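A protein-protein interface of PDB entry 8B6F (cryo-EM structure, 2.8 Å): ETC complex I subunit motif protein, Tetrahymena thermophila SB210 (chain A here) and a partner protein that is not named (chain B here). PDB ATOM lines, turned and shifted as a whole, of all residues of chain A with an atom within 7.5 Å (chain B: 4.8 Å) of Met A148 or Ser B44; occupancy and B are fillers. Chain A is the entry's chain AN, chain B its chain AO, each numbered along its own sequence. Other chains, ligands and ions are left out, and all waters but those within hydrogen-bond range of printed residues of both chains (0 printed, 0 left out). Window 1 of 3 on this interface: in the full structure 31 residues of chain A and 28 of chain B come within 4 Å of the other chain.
OG of Ser B44 sits at hydrogen-bond distance from O of Trp B41. O of Tyr A147 lies within hydrogen-bond range of OG of Ser A151 (3.2 Å).
Among the printed residues, merely in contact across the chains: Arg A157 with Trp B41 (3.3 Å), Arg A157 with Ser B44 (3.6 Å), Pro A153 with Phe B15 (3.6 Å), Pro A153 with Trp B41 (3.7 Å), Leu A144 with Leu B47 (3.8 Å), Tyr A147 with Leu B47 (3.9 Å), Ser A151 with Ser B44 (3.9 Å), Leu A144 with Phe B48 (3.9 Å), Met A148 with Ser B44 (3.9 Å) and Met A148 with Phe B48 (3.96 Å).
Of the printed residues of chain B, Tyr A147 touches Leu B47. His A150 touches none of the printed residues of chain B. Printed residues of chain B within 4 Å of Ser A151: Ser B44 (3.9 Å). Printed residues of chain B within 4 Å of Pro A153: Phe B15 (3.6 Å) and Trp B41 (3.7 Å). Printed residues of chain B within 4 Å of Arg A157: Trp B41 and Ser B44. Of the printed residues of chain A, Phe B15 touches Pro A153. Ser B44 touches just these residues of chain A: Met A148, Ser A151 and Arg A157. The nearest residue of chain B that does not touch Met A148 is Leu B47 (4.2 Å). The nearest printed residue of chain A that does not touch Trp B41 is Lys A152 (4.2 Å).
Hydrophobic or aromatic side chains of chain B within 4 Å of the printed part of chain A: Phe B15, Trp B41, Leu B47 and Phe B48. Of the 18 printed residues of chain A, 6 touch a printed residue of chain B. Printed residues of chain A that touch a printed residue of chain B: Leu A144, Tyr A147, Met A148, Ser A151, Pro A153 and Arg A157. Among the printed residues, 10 pairs touch across the chains. Among the printed residues, no Asp or Glu carboxylate lies within 4 Å of a Lys or Arg side-chain nitrogen of the other chain.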
ATOM      1  N   LEU A  89       8.370 -12.791  14.202  1.00  0.00           N
ATOM      2  CA  LEU A  89       8.889 -12.474  15.527  1.00  0.00           C
ATOM      3  C   LEU A  89      10.358 -12.076  15.514  1.00  0.00           C
ATOM      4  O   LEU A  89      10.844 -11.554  16.523  1.00  0.00           O
ATOM      5  CB  LEU A  89       8.702 -13.664  16.470  1.00  0.00           C
ATOM      6  CG  LEU A  89       7.315 -13.863  17.088  1.00  0.00           C
ATOM      7  CD1 LEU A  89       7.305 -15.128  17.919  1.00  0.00           C
ATOM      8  CD2 LEU A  89       6.900 -12.672  17.938  1.00  0.00           C
ATOM      9  N   ILE A  92      11.292  -8.440  16.581  1.00  0.00           N
ATOM     10  CA  ILE A  92      11.300  -8.111  18.003  1.00  0.00           C
ATOM     11  C   ILE A  92      12.644  -8.544  18.580  1.00  0.00           C
ATOM     12  O   ILE A  92      13.204  -9.553  18.130  1.00  0.00           O
ATOM     13  CB  ILE A  92      10.120  -8.778  18.731  1.00  0.00           C
ATOM     14  CG1 ILE A  92       8.794  -8.097  18.370  1.00  0.00           C
ATOM     15  CG2 ILE A  92      10.299  -8.738  20.240  1.00  0.00           C
ATOM     16  CD1 ILE A  92       8.321  -8.311  16.944  1.00  0.00           C
ATOM     17  N   TYR A  98       7.950 -10.662  25.369  1.00  0.00           N
ATOM     18  CA  TYR A  98       6.866 -10.914  24.428  1.00  0.00           C
ATOM     19  C   TYR A  98       7.286 -11.947  23.391  1.00  0.00           C
ATOM     20  O   TYR A  98       6.535 -12.881  23.088  1.00  0.00           O
ATOM     21  CB  TYR A  98       6.446  -9.610  23.749  1.00  0.00           C
ATOM     22  CG  TYR A  98       5.558  -9.827  22.550  1.00  0.00           C
ATOM     23  CD1 TYR A  98       4.254 -10.279  22.705  1.00  0.00           C
ATOM     24  CD2 TYR A  98       6.018  -9.580  21.265  1.00  0.00           C
ATOM     25  CE1 TYR A  98       3.437 -10.483  21.615  1.00  0.00           C
ATOM     26  CE2 TYR A  98       5.208  -9.781  20.166  1.00  0.00           C
ATOM     27  CZ  TYR A  98       3.919 -10.234  20.349  1.00  0.00           C
ATOM     28  OH  TYR A  98       3.104 -10.435  19.263  1.00  0.00           O
ATOM     29  N   THR A 102       5.636 -15.671  23.025  1.00  0.00           N
ATOM     30  CA  THR A 102       4.996 -16.061  21.773  1.00  0.00           C
ATOM     31  C   THR A 102       5.680 -17.271  21.150  1.00  0.00           C
ATOM     32  O   THR A 102       5.010 -18.172  20.637  1.00  0.00           O
ATOM     33  CB  THR A 102       4.993 -14.891  20.792  1.00  0.00           C
ATOM     34  OG1 THR A 102       4.506 -13.715  21.448  1.00  0.00           O
ATOM     35  CG2 THR A 102       4.097 -15.200  19.602  1.00  0.00           C
ATOM     36  N   GLU A 141      -2.574 -13.091  15.773  1.00  0.00           N
ATOM     37  CA  GLU A 141      -1.229 -12.819  16.264  1.00  0.00           C
ATOM     38  C   GLU A 141      -0.333 -12.270  15.163  1.00  0.00           C
ATOM     39  O   GLU A 141       0.605 -11.520  15.449  1.00  0.00           O
ATOM     40  CB  GLU A 141      -0.624 -14.078  16.879  1.00  0.00           C
ATOM     41  CG  GLU A 141      -1.356 -14.535  18.132  1.00  0.00           C
ATOM     42  CD  GLU A 141      -0.621 -15.631  18.875  1.00  0.00           C
ATOM     43  OE1 GLU A 141       0.372 -16.158  18.333  1.00  0.00           O
ATOM     44  OE2 GLU A 141      -1.033 -15.960  20.007  1.00  0.00           O
ATOM     45  N   GLU A 143      -1.100  -9.986  13.002  1.00  0.00           N
ATOM     46  CA  GLU A 143      -1.241  -8.538  13.095  1.00  0.00           C
ATOM     47  C   GLU A 143      -0.756  -8.005  14.436  1.00  0.00           C
ATOM     48  O   GLU A 143      -0.223  -6.892  14.497  1.00  0.00           O
ATOM     49  CB  GLU A 143      -2.700  -8.132  12.869  1.00  0.00           C
ATOM     50  CG  GLU A 143      -3.229  -8.434  11.471  1.00  0.00           C
ATOM     51  CD  GLU A 143      -3.506  -9.910  11.242  1.00  0.00           C
ATOM     52  OE1 GLU A 143      -3.590 -10.663  12.234  1.00  0.00           O
ATOM     53  OE2 GLU A 143      -3.636 -10.319  10.069  1.00  0.00           O
ATOM     54  N   LEU A 144      -0.926  -8.774  15.511  1.00  0.00           N
ATOM     55  CA  LEU A 144      -0.489  -8.315  16.825  1.00  0.00           C
ATOM     56  C   LEU A 144       1.020  -8.121  16.885  1.00  0.00           C
ATOM     57  O   LEU A 144       1.507  -7.315  17.685  1.00  0.00           O
ATOM     58  CB  LEU A 144      -0.934  -9.311  17.896  1.00  0.00           C
ATOM     59  CG  LEU A 144      -0.428  -9.067  19.319  1.00  0.00           C
ATOM     60  CD1 LEU A 144      -0.876  -7.711  19.827  1.00  0.00           C
ATOM     61  CD2 LEU A 144      -0.904 -10.170  20.245  1.00  0.00           C
ATOM     62  N   VAL A 145       1.778  -8.848  16.060  1.00  0.00           N
ATOM     63  CA  VAL A 145       3.236  -8.760  16.123  1.00  0.00           C
ATOM     64  C   VAL A 145       3.696  -7.333  15.854  1.00  0.00           C
ATOM     65  O   VAL A 145       4.529  -6.783  16.584  1.00  0.00           O
ATOM     66  CB  VAL A 145       3.883  -9.757  15.142  1.00  0.00           C
ATOM     67  CG1 VAL A 145       5.354  -9.435  14.929  1.00  0.00           C
ATOM     68  CG2 VAL A 145       3.751 -11.175  15.666  1.00  0.00           C
ATOM     69  N   GLU A 146       3.163  -6.710  14.803  1.00  0.00           N
ATOM     70  CA  GLU A 146       3.591  -5.357  14.467  1.00  0.00           C
ATOM     71  C   GLU A 146       3.118  -4.352  15.508  1.00  0.00           C
ATOM     72  O   GLU A 146       3.836  -3.399  15.828  1.00  0.00           O
ATOM     73  CB  GLU A 146       3.083  -4.971  13.080  1.00  0.00           C
ATOM     74  CG  GLU A 146       3.602  -3.623  12.606  1.00  0.00           C
ATOM     75  CD  GLU A 146       3.273  -3.349  11.155  1.00  0.00           C
ATOM     76  OE1 GLU A 146       2.671  -4.229  10.506  1.00  0.00           O
ATOM     77  OE2 GLU A 146       3.616  -2.253  10.663  1.00  0.00           O
ATOM     78  N   TYR A 147       1.909  -4.538  16.041  1.00  0.00           N
ATOM     79  CA  TYR A 147       1.429  -3.657  17.099  1.00  0.00           C
ATOM     80  C   TYR A 147       2.358  -3.691  18.304  1.00  0.00           C
ATOM     81  O   TYR A 147       2.715  -2.646  18.859  1.00  0.00           O
ATOM     82  CB  TYR A 147       0.015  -4.052  17.518  1.00  0.00           C
ATOM     83  CG  TYR A 147      -1.064  -3.476  16.646  1.00  0.00           C
ATOM     84  CD1 TYR A 147      -1.352  -2.121  16.684  1.00  0.00           C
ATOM     85  CD2 TYR A 147      -1.812  -4.285  15.809  1.00  0.00           C
ATOM     86  CE1 TYR A 147      -2.342  -1.584  15.900  1.00  0.00           C
ATOM     87  CE2 TYR A 147      -2.806  -3.756  15.019  1.00  0.00           C
ATOM     88  CZ  TYR A 147      -3.067  -2.406  15.073  1.00  0.00           C
ATOM     89  OH  TYR A 147      -4.054  -1.878  14.289  1.00  0.00           O
ATOM     90  N   MET A 148       2.765  -4.890  18.721  1.00  0.00           N
ATOM     91  CA  MET A 148       3.667  -5.006  19.860  1.00  0.00           C
ATOM     92  C   MET A 148       5.054  -4.479  19.527  1.00  0.00           C
ATOM     93  O   MET A 148       5.729  -3.923  20.399  1.00  0.00           O
ATOM     94  CB  MET A 148       3.746  -6.460  20.322  1.00  0.00           C
ATOM     95  CG  MET A 148       2.468  -6.971  20.970  1.00  0.00           C
ATOM     96  SD  MET A 148       1.989  -6.050  22.445  1.00  0.00           S
ATOM     97  CE  MET A 148       0.763  -4.928  21.775  1.00  0.00           C
ATOM     98  N   LYS A 149       5.494  -4.639  18.279  1.00  0.00           N
ATOM     99  CA  LYS A 149       6.775  -4.071  17.877  1.00  0.00           C
ATOM    100  C   LYS A 149       6.769  -2.555  18.027  1.00  0.00           C
ATOM    101  O   LYS A 149       7.754  -1.966  18.485  1.00  0.00           O
ATOM    102  CB  LYS A 149       7.085  -4.471  16.434  1.00  0.00           C
ATOM    103  CG  LYS A 149       8.318  -3.804  15.847  1.00  0.00           C
ATOM    104  CD  LYS A 149       8.621  -4.319  14.446  1.00  0.00           C
ATOM    105  CE  LYS A 149       7.520  -3.958  13.459  1.00  0.00           C
ATOM    106  NZ  LYS A 149       7.858  -4.370  12.065  1.00  0.00           N
ATOM    107  N   HIS A 150       5.674  -1.904  17.633  1.00  0.00           N
ATOM    108  CA  HIS A 150       5.606  -0.451  17.742  1.00  0.00           C
ATOM    109  C   HIS A 150       5.415  -0.006  19.187  1.00  0.00           C
ATOM    110  O   HIS A 150       5.982   1.008  19.607  1.00  0.00           O
ATOM    111  CB  HIS A 150       4.484   0.085  16.855  1.00  0.00           C
ATOM    112  CG  HIS A 150       4.834   0.116  15.401  1.00  0.00           C
ATOM    113  ND1 HIS A 150       4.834  -1.014  14.611  1.00  0.00           N
ATOM    114  CD2 HIS A 150       5.207   1.137  14.595  1.00  0.00           C
ATOM    115  CE1 HIS A 150       5.186  -0.689  13.380  1.00  0.00           C
ATOM    116  NE2 HIS A 150       5.420   0.611  13.344  1.00  0.00           N
ATOM    117  N   SER A 151       4.613  -0.742  19.960  1.00  0.00           N
ATOM    118  CA  SER A 151       4.396  -0.368  21.354  1.00  0.00           C
ATOM    119  C   SER A 151       5.667  -0.537  22.177  1.00  0.00           C
ATOM    120  O   SER A 151       5.937   0.260  23.083  1.00  0.00           O
ATOM    121  CB  SER A 151       3.261  -1.196  21.955  1.00  0.00           C
ATOM    122  OG  SER A 151       2.013  -0.832  21.396  1.00  0.00           O
ATOM    123  N   LYS A 152       6.453  -1.571  21.883  1.00  0.00           N
ATOM    124  CA  LYS A 152       7.695  -1.833  22.598  1.00  0.00           C
ATOM    125  C   LYS A 152       7.420  -2.056  24.080  1.00  0.00           C
ATOM    126  O   LYS A 152       7.847  -1.252  24.919  1.00  0.00           O
ATOM    127  CB  LYS A 152       8.683  -0.681  22.404  1.00  0.00           C
ATOM    128  CG  LYS A 152       9.006  -0.398  20.945  1.00  0.00           C
ATOM    129  CD  LYS A 152       9.980   0.757  20.805  1.00  0.00           C
ATOM    130  CE  LYS A 152      10.282   1.035  19.341  1.00  0.00           C
ATOM    131  NZ  LYS A 152      11.241   2.161  19.172  1.00  0.00           N
ATOM    132  N   PRO A 153       6.720  -3.132  24.444  1.00  0.00           N
ATOM    133  CA  PRO A 153       6.476  -3.397  25.871  1.00  0.00           C
ATOM    134  C   PRO A 153       7.741  -3.654  26.669  1.00  0.00           C
ATOM    135  O   PRO A 153       7.700  -3.580  27.902  1.00  0.00           O
ATOM    136  CB  PRO A 153       5.560  -4.630  25.849  1.00  0.00           C
ATOM    137  CG  PRO A 153       5.793  -5.261  24.527  1.00  0.00           C
ATOM    138  CD  PRO A 153       6.093  -4.144  23.579  1.00  0.00           C
ATOM    139  N   TRP A 154       8.858  -3.959  26.012  1.00  0.00           N
ATOM    140  CA  TRP A 154      10.107  -4.251  26.703  1.00  0.00           C
ATOM    141  C   TRP A 154      10.863  -3.002  27.138  1.00  0.00           C
ATOM    142  O   TRP A 154      11.897  -3.129  27.802  1.00  0.00           O
ATOM    143  CB  TRP A 154      11.008  -5.109  25.810  1.00  0.00           C
ATOM    144  CG  TRP A 154      11.272  -4.515  24.465  1.00  0.00           C
ATOM    145  CD1 TRP A 154      12.270  -3.650  24.133  1.00  0.00           C
ATOM    146  CD2 TRP A 154      10.523  -4.745  23.264  1.00  0.00           C
ATOM    147  NE1 TRP A 154      12.191  -3.326  22.801  1.00  0.00           N
ATOM    148  CE2 TRP A 154      11.126  -3.984  22.245  1.00  0.00           C
ATOM    149  CE3 TRP A 154       9.401  -5.520  22.954  1.00  0.00           C
ATOM    150  CZ2 TRP A 154      10.647  -3.976  20.937  1.00  0.00           C
ATOM    151  CZ3 TRP A 154       8.926  -5.512  21.655  1.00  0.00           C
ATOM    152  CH2 TRP A 154       9.548  -4.744  20.662  1.00  0.00           C
ATOM    153  N   ARG A 157       8.403   3.498  29.953  1.00  0.00           N
ATOM    154  CA  ARG A 157       7.853   4.811  29.663  1.00  0.00           C
ATOM    155  C   ARG A 157       8.117   5.769  30.817  1.00  0.00           C
ATOM    156  O   ARG A 157       8.380   5.344  31.947  1.00  0.00           O
ATOM    157  CB  ARG A 157       6.353   4.710  29.401  1.00  0.00           C
ATOM    158  CG  ARG A 157       5.979   3.769  28.266  1.00  0.00           C
ATOM    159  CD  ARG A 157       4.492   3.852  27.961  1.00  0.00           C
ATOM    160  NE  ARG A 157       3.980   2.630  27.354  1.00  0.00           N
ATOM    161  CZ  ARG A 157       4.091   2.322  26.070  1.00  0.00           C
ATOM    162  NH1 ARG A 157       4.712   3.121  25.220  1.00  0.00           N
ATOM    163  NH2 ARG A 157       3.567   1.184  25.628  1.00  0.00           N
ATOM    164  N   PHE B  15       4.152  -7.661  29.316  1.00  0.00           N
ATOM    165  CA  PHE B  15       4.566  -6.305  29.674  1.00  0.00           C
ATOM    166  C   PHE B  15       5.491  -6.411  30.882  1.00  0.00           C
ATOM    167  O   PHE B  15       5.096  -6.246  32.039  1.00  0.00           O
ATOM    168  CB  PHE B  15       3.350  -5.429  29.943  1.00  0.00           C
ATOM    169  CG  PHE B  15       2.487  -5.213  28.734  1.00  0.00           C
ATOM    170  CD1 PHE B  15       1.524  -6.139  28.376  1.00  0.00           C
ATOM    171  CD2 PHE B  15       2.650  -4.087  27.948  1.00  0.00           C
ATOM    172  CE1 PHE B  15       0.736  -5.944  27.259  1.00  0.00           C
ATOM    173  CE2 PHE B  15       1.867  -3.885  26.830  1.00  0.00           C
ATOM    174  CZ  PHE B  15       0.908  -4.815  26.485  1.00  0.00           C
ATOM    175  N   TRP B  41       0.145   2.601  30.115  1.00  0.00           N
ATOM    176  CA  TRP B  41       0.202   1.306  29.453  1.00  0.00           C
ATOM    177  C   TRP B  41      -1.175   0.760  29.107  1.00  0.00           C
ATOM    178  O   TRP B  41      -1.265  -0.311  28.501  1.00  0.00           O
ATOM    179  CB  TRP B  41       0.936   0.292  30.337  1.00  0.00           C
ATOM    180  CG  TRP B  41       2.384   0.584  30.537  1.00  0.00           C
ATOM    181  CD1 TRP B  41       2.945   1.284  31.562  1.00  0.00           C
ATOM    182  CD2 TRP B  41       3.462   0.173  29.693  1.00  0.00           C
ATOM    183  NE1 TRP B  41       4.309   1.335  31.408  1.00  0.00           N
ATOM    184  CE2 TRP B  41       4.651   0.660  30.266  1.00  0.00           C
ATOM    185  CE3 TRP B  41       3.536  -0.562  28.507  1.00  0.00           C
ATOM    186  CZ2 TRP B  41       5.900   0.438  29.694  1.00  0.00           C
ATOM    187  CZ3 TRP B  41       4.774  -0.781  27.939  1.00  0.00           C
ATOM    188  CH2 TRP B  41       5.941  -0.284  28.533  1.00  0.00           C
ATOM    189  N   PHE B  42      -2.247   1.466  29.475  1.00  0.00           N
ATOM    190  CA  PHE B  42      -3.593   0.953  29.247  1.00  0.00           C
ATOM    191  C   PHE B  42      -3.851   0.678  27.770  1.00  0.00           C
ATOM    192  O   PHE B  42      -4.410  -0.366  27.416  1.00  0.00           O
ATOM    193  CB  PHE B  42      -4.617   1.944  29.800  1.00  0.00           C
ATOM    194  CG  PHE B  42      -6.035   1.470  29.701  1.00  0.00           C
ATOM    195  CD1 PHE B  42      -6.496   0.451  30.517  1.00  0.00           C
ATOM    196  CD2 PHE B  42      -6.915   2.060  28.811  1.00  0.00           C
ATOM    197  CE1 PHE B  42      -7.804   0.019  30.436  1.00  0.00           C
ATOM    198  CE2 PHE B  42      -8.224   1.632  28.726  1.00  0.00           C
ATOM    199  CZ  PHE B  42      -8.668   0.610  29.540  1.00  0.00           C
ATOM    200  N   TYR B  43      -3.462   1.602  26.891  1.00  0.00           N
ATOM    201  CA  TYR B  43      -3.759   1.436  25.470  1.00  0.00           C
ATOM    202  C   TYR B  43      -3.027   0.235  24.883  1.00  0.00           C
ATOM    203  O   TYR B  43      -3.622  -0.576  24.164  1.00  0.00           O
ATOM    204  CB  TYR B  43      -3.401   2.706  24.703  1.00  0.00           C
ATOM    205  CG  TYR B  43      -3.732   2.619  23.233  1.00  0.00           C
ATOM    206  CD1 TYR B  43      -5.020   2.855  22.776  1.00  0.00           C
ATOM    207  CD2 TYR B  43      -2.755   2.301  22.301  1.00  0.00           C
ATOM    208  CE1 TYR B  43      -5.327   2.774  21.433  1.00  0.00           C
ATOM    209  CE2 TYR B  43      -3.050   2.217  20.957  1.00  0.00           C
ATOM    210  CZ  TYR B  43      -4.337   2.456  20.529  1.00  0.00           C
ATOM    211  OH  TYR B  43      -4.634   2.373  19.189  1.00  0.00           O
ATOM    212  N   SER B  44      -1.733   0.101  25.178  1.00  0.00           N
ATOM    213  CA  SER B  44      -0.974  -1.040  24.675  1.00  0.00           C
ATOM    214  C   SER B  44      -1.509  -2.348  25.241  1.00  0.00           C
ATOM    215  O   SER B  44      -1.558  -3.364  24.541  1.00  0.00           O
ATOM    216  CB  SER B  44       0.507  -0.880  25.013  1.00  0.00           C
ATOM    217  OG  SER B  44       0.707  -0.845  26.415  1.00  0.00           O
ATOM    218  N   ILE B  45      -1.920  -2.339  26.509  1.00  0.00           N
ATOM    219  CA  ILE B  45      -2.466  -3.545  27.123  1.00  0.00           C
ATOM    220  C   ILE B  45      -3.752  -3.961  26.424  1.00  0.00           C
ATOM    221  O   ILE B  45      -3.984  -5.151  26.179  1.00  0.00           O
ATOM    222  CB  ILE B  45      -2.670  -3.319  28.631  1.00  0.00           C
ATOM    223  CG1 ILE B  45      -1.305  -3.262  29.318  1.00  0.00           C
ATOM    224  CG2 ILE B  45      -3.550  -4.400  29.241  1.00  0.00           C
ATOM    225  CD1 ILE B  45      -1.335  -2.650  30.671  1.00  0.00           C
ATOM    226  N   ASN B  46      -4.606  -2.997  26.090  1.00  0.00           N
ATOM    227  CA  ASN B  46      -5.823  -3.323  25.355  1.00  0.00           C
ATOM    228  C   ASN B  46      -5.499  -3.812  23.951  1.00  0.00           C
ATOM    229  O   ASN B  46      -6.185  -4.692  23.422  1.00  0.00           O
ATOM    230  CB  ASN B  46      -6.750  -2.114  25.312  1.00  0.00           C
ATOM    231  CG  ASN B  46      -7.524  -1.943  26.596  1.00  0.00           C
ATOM    232  OD1 ASN B  46      -8.712  -2.255  26.665  1.00  0.00           O
ATOM    233  ND2 ASN B  46      -6.849  -1.467  27.632  1.00  0.00           N
ATOM    234  N   LEU B  47      -4.468  -3.246  23.323  1.00  0.00           N
ATOM    235  CA  LEU B  47      -4.039  -3.750  22.023  1.00  0.00           C
ATOM    236  C   LEU B  47      -3.652  -5.220  22.118  1.00  0.00           C
ATOM    237  O   LEU B  47      -4.028  -6.031  21.264  1.00  0.00           O
ATOM    238  CB  LEU B  47      -2.863  -2.926  21.495  1.00  0.00           C
ATOM    239  CG  LEU B  47      -3.158  -1.633  20.730  1.00  0.00           C
ATOM    240  CD1 LEU B  47      -1.854  -0.950  20.357  1.00  0.00           C
ATOM    241  CD2 LEU B  47      -3.992  -1.891  19.490  1.00  0.00           C
ATOM    242  N   PHE B  48      -2.890  -5.579  23.150  1.00  0.00           N
ATOM    243  CA  PHE B  48      -2.501  -6.972  23.333  1.00  0.00           C
ATOM    244  C   PHE B  48      -3.712  -7.851  23.618  1.00  0.00           C
ATOM    245  O   PHE B  48      -3.813  -8.966  23.092  1.00  0.00           O
ATOM    246  CB  PHE B  48      -1.478  -7.083  24.462  1.00  0.00           C
ATOM    247  CG  PHE B  48      -1.058  -8.491  24.755  1.00  0.00           C
ATOM    248  CD1 PHE B  48      -0.047  -9.089  24.026  1.00  0.00           C
ATOM    249  CD2 PHE B  48      -1.676  -9.218  25.759  1.00  0.00           C
ATOM    250  CE1 PHE B  48       0.342 -10.384  24.293  1.00  0.00           C
ATOM    251  CE2 PHE B  48      -1.291 -10.514  26.029  1.00  0.00           C
ATOM    252  CZ  PHE B  48      -0.283 -11.097  25.295  1.00  0.00           C
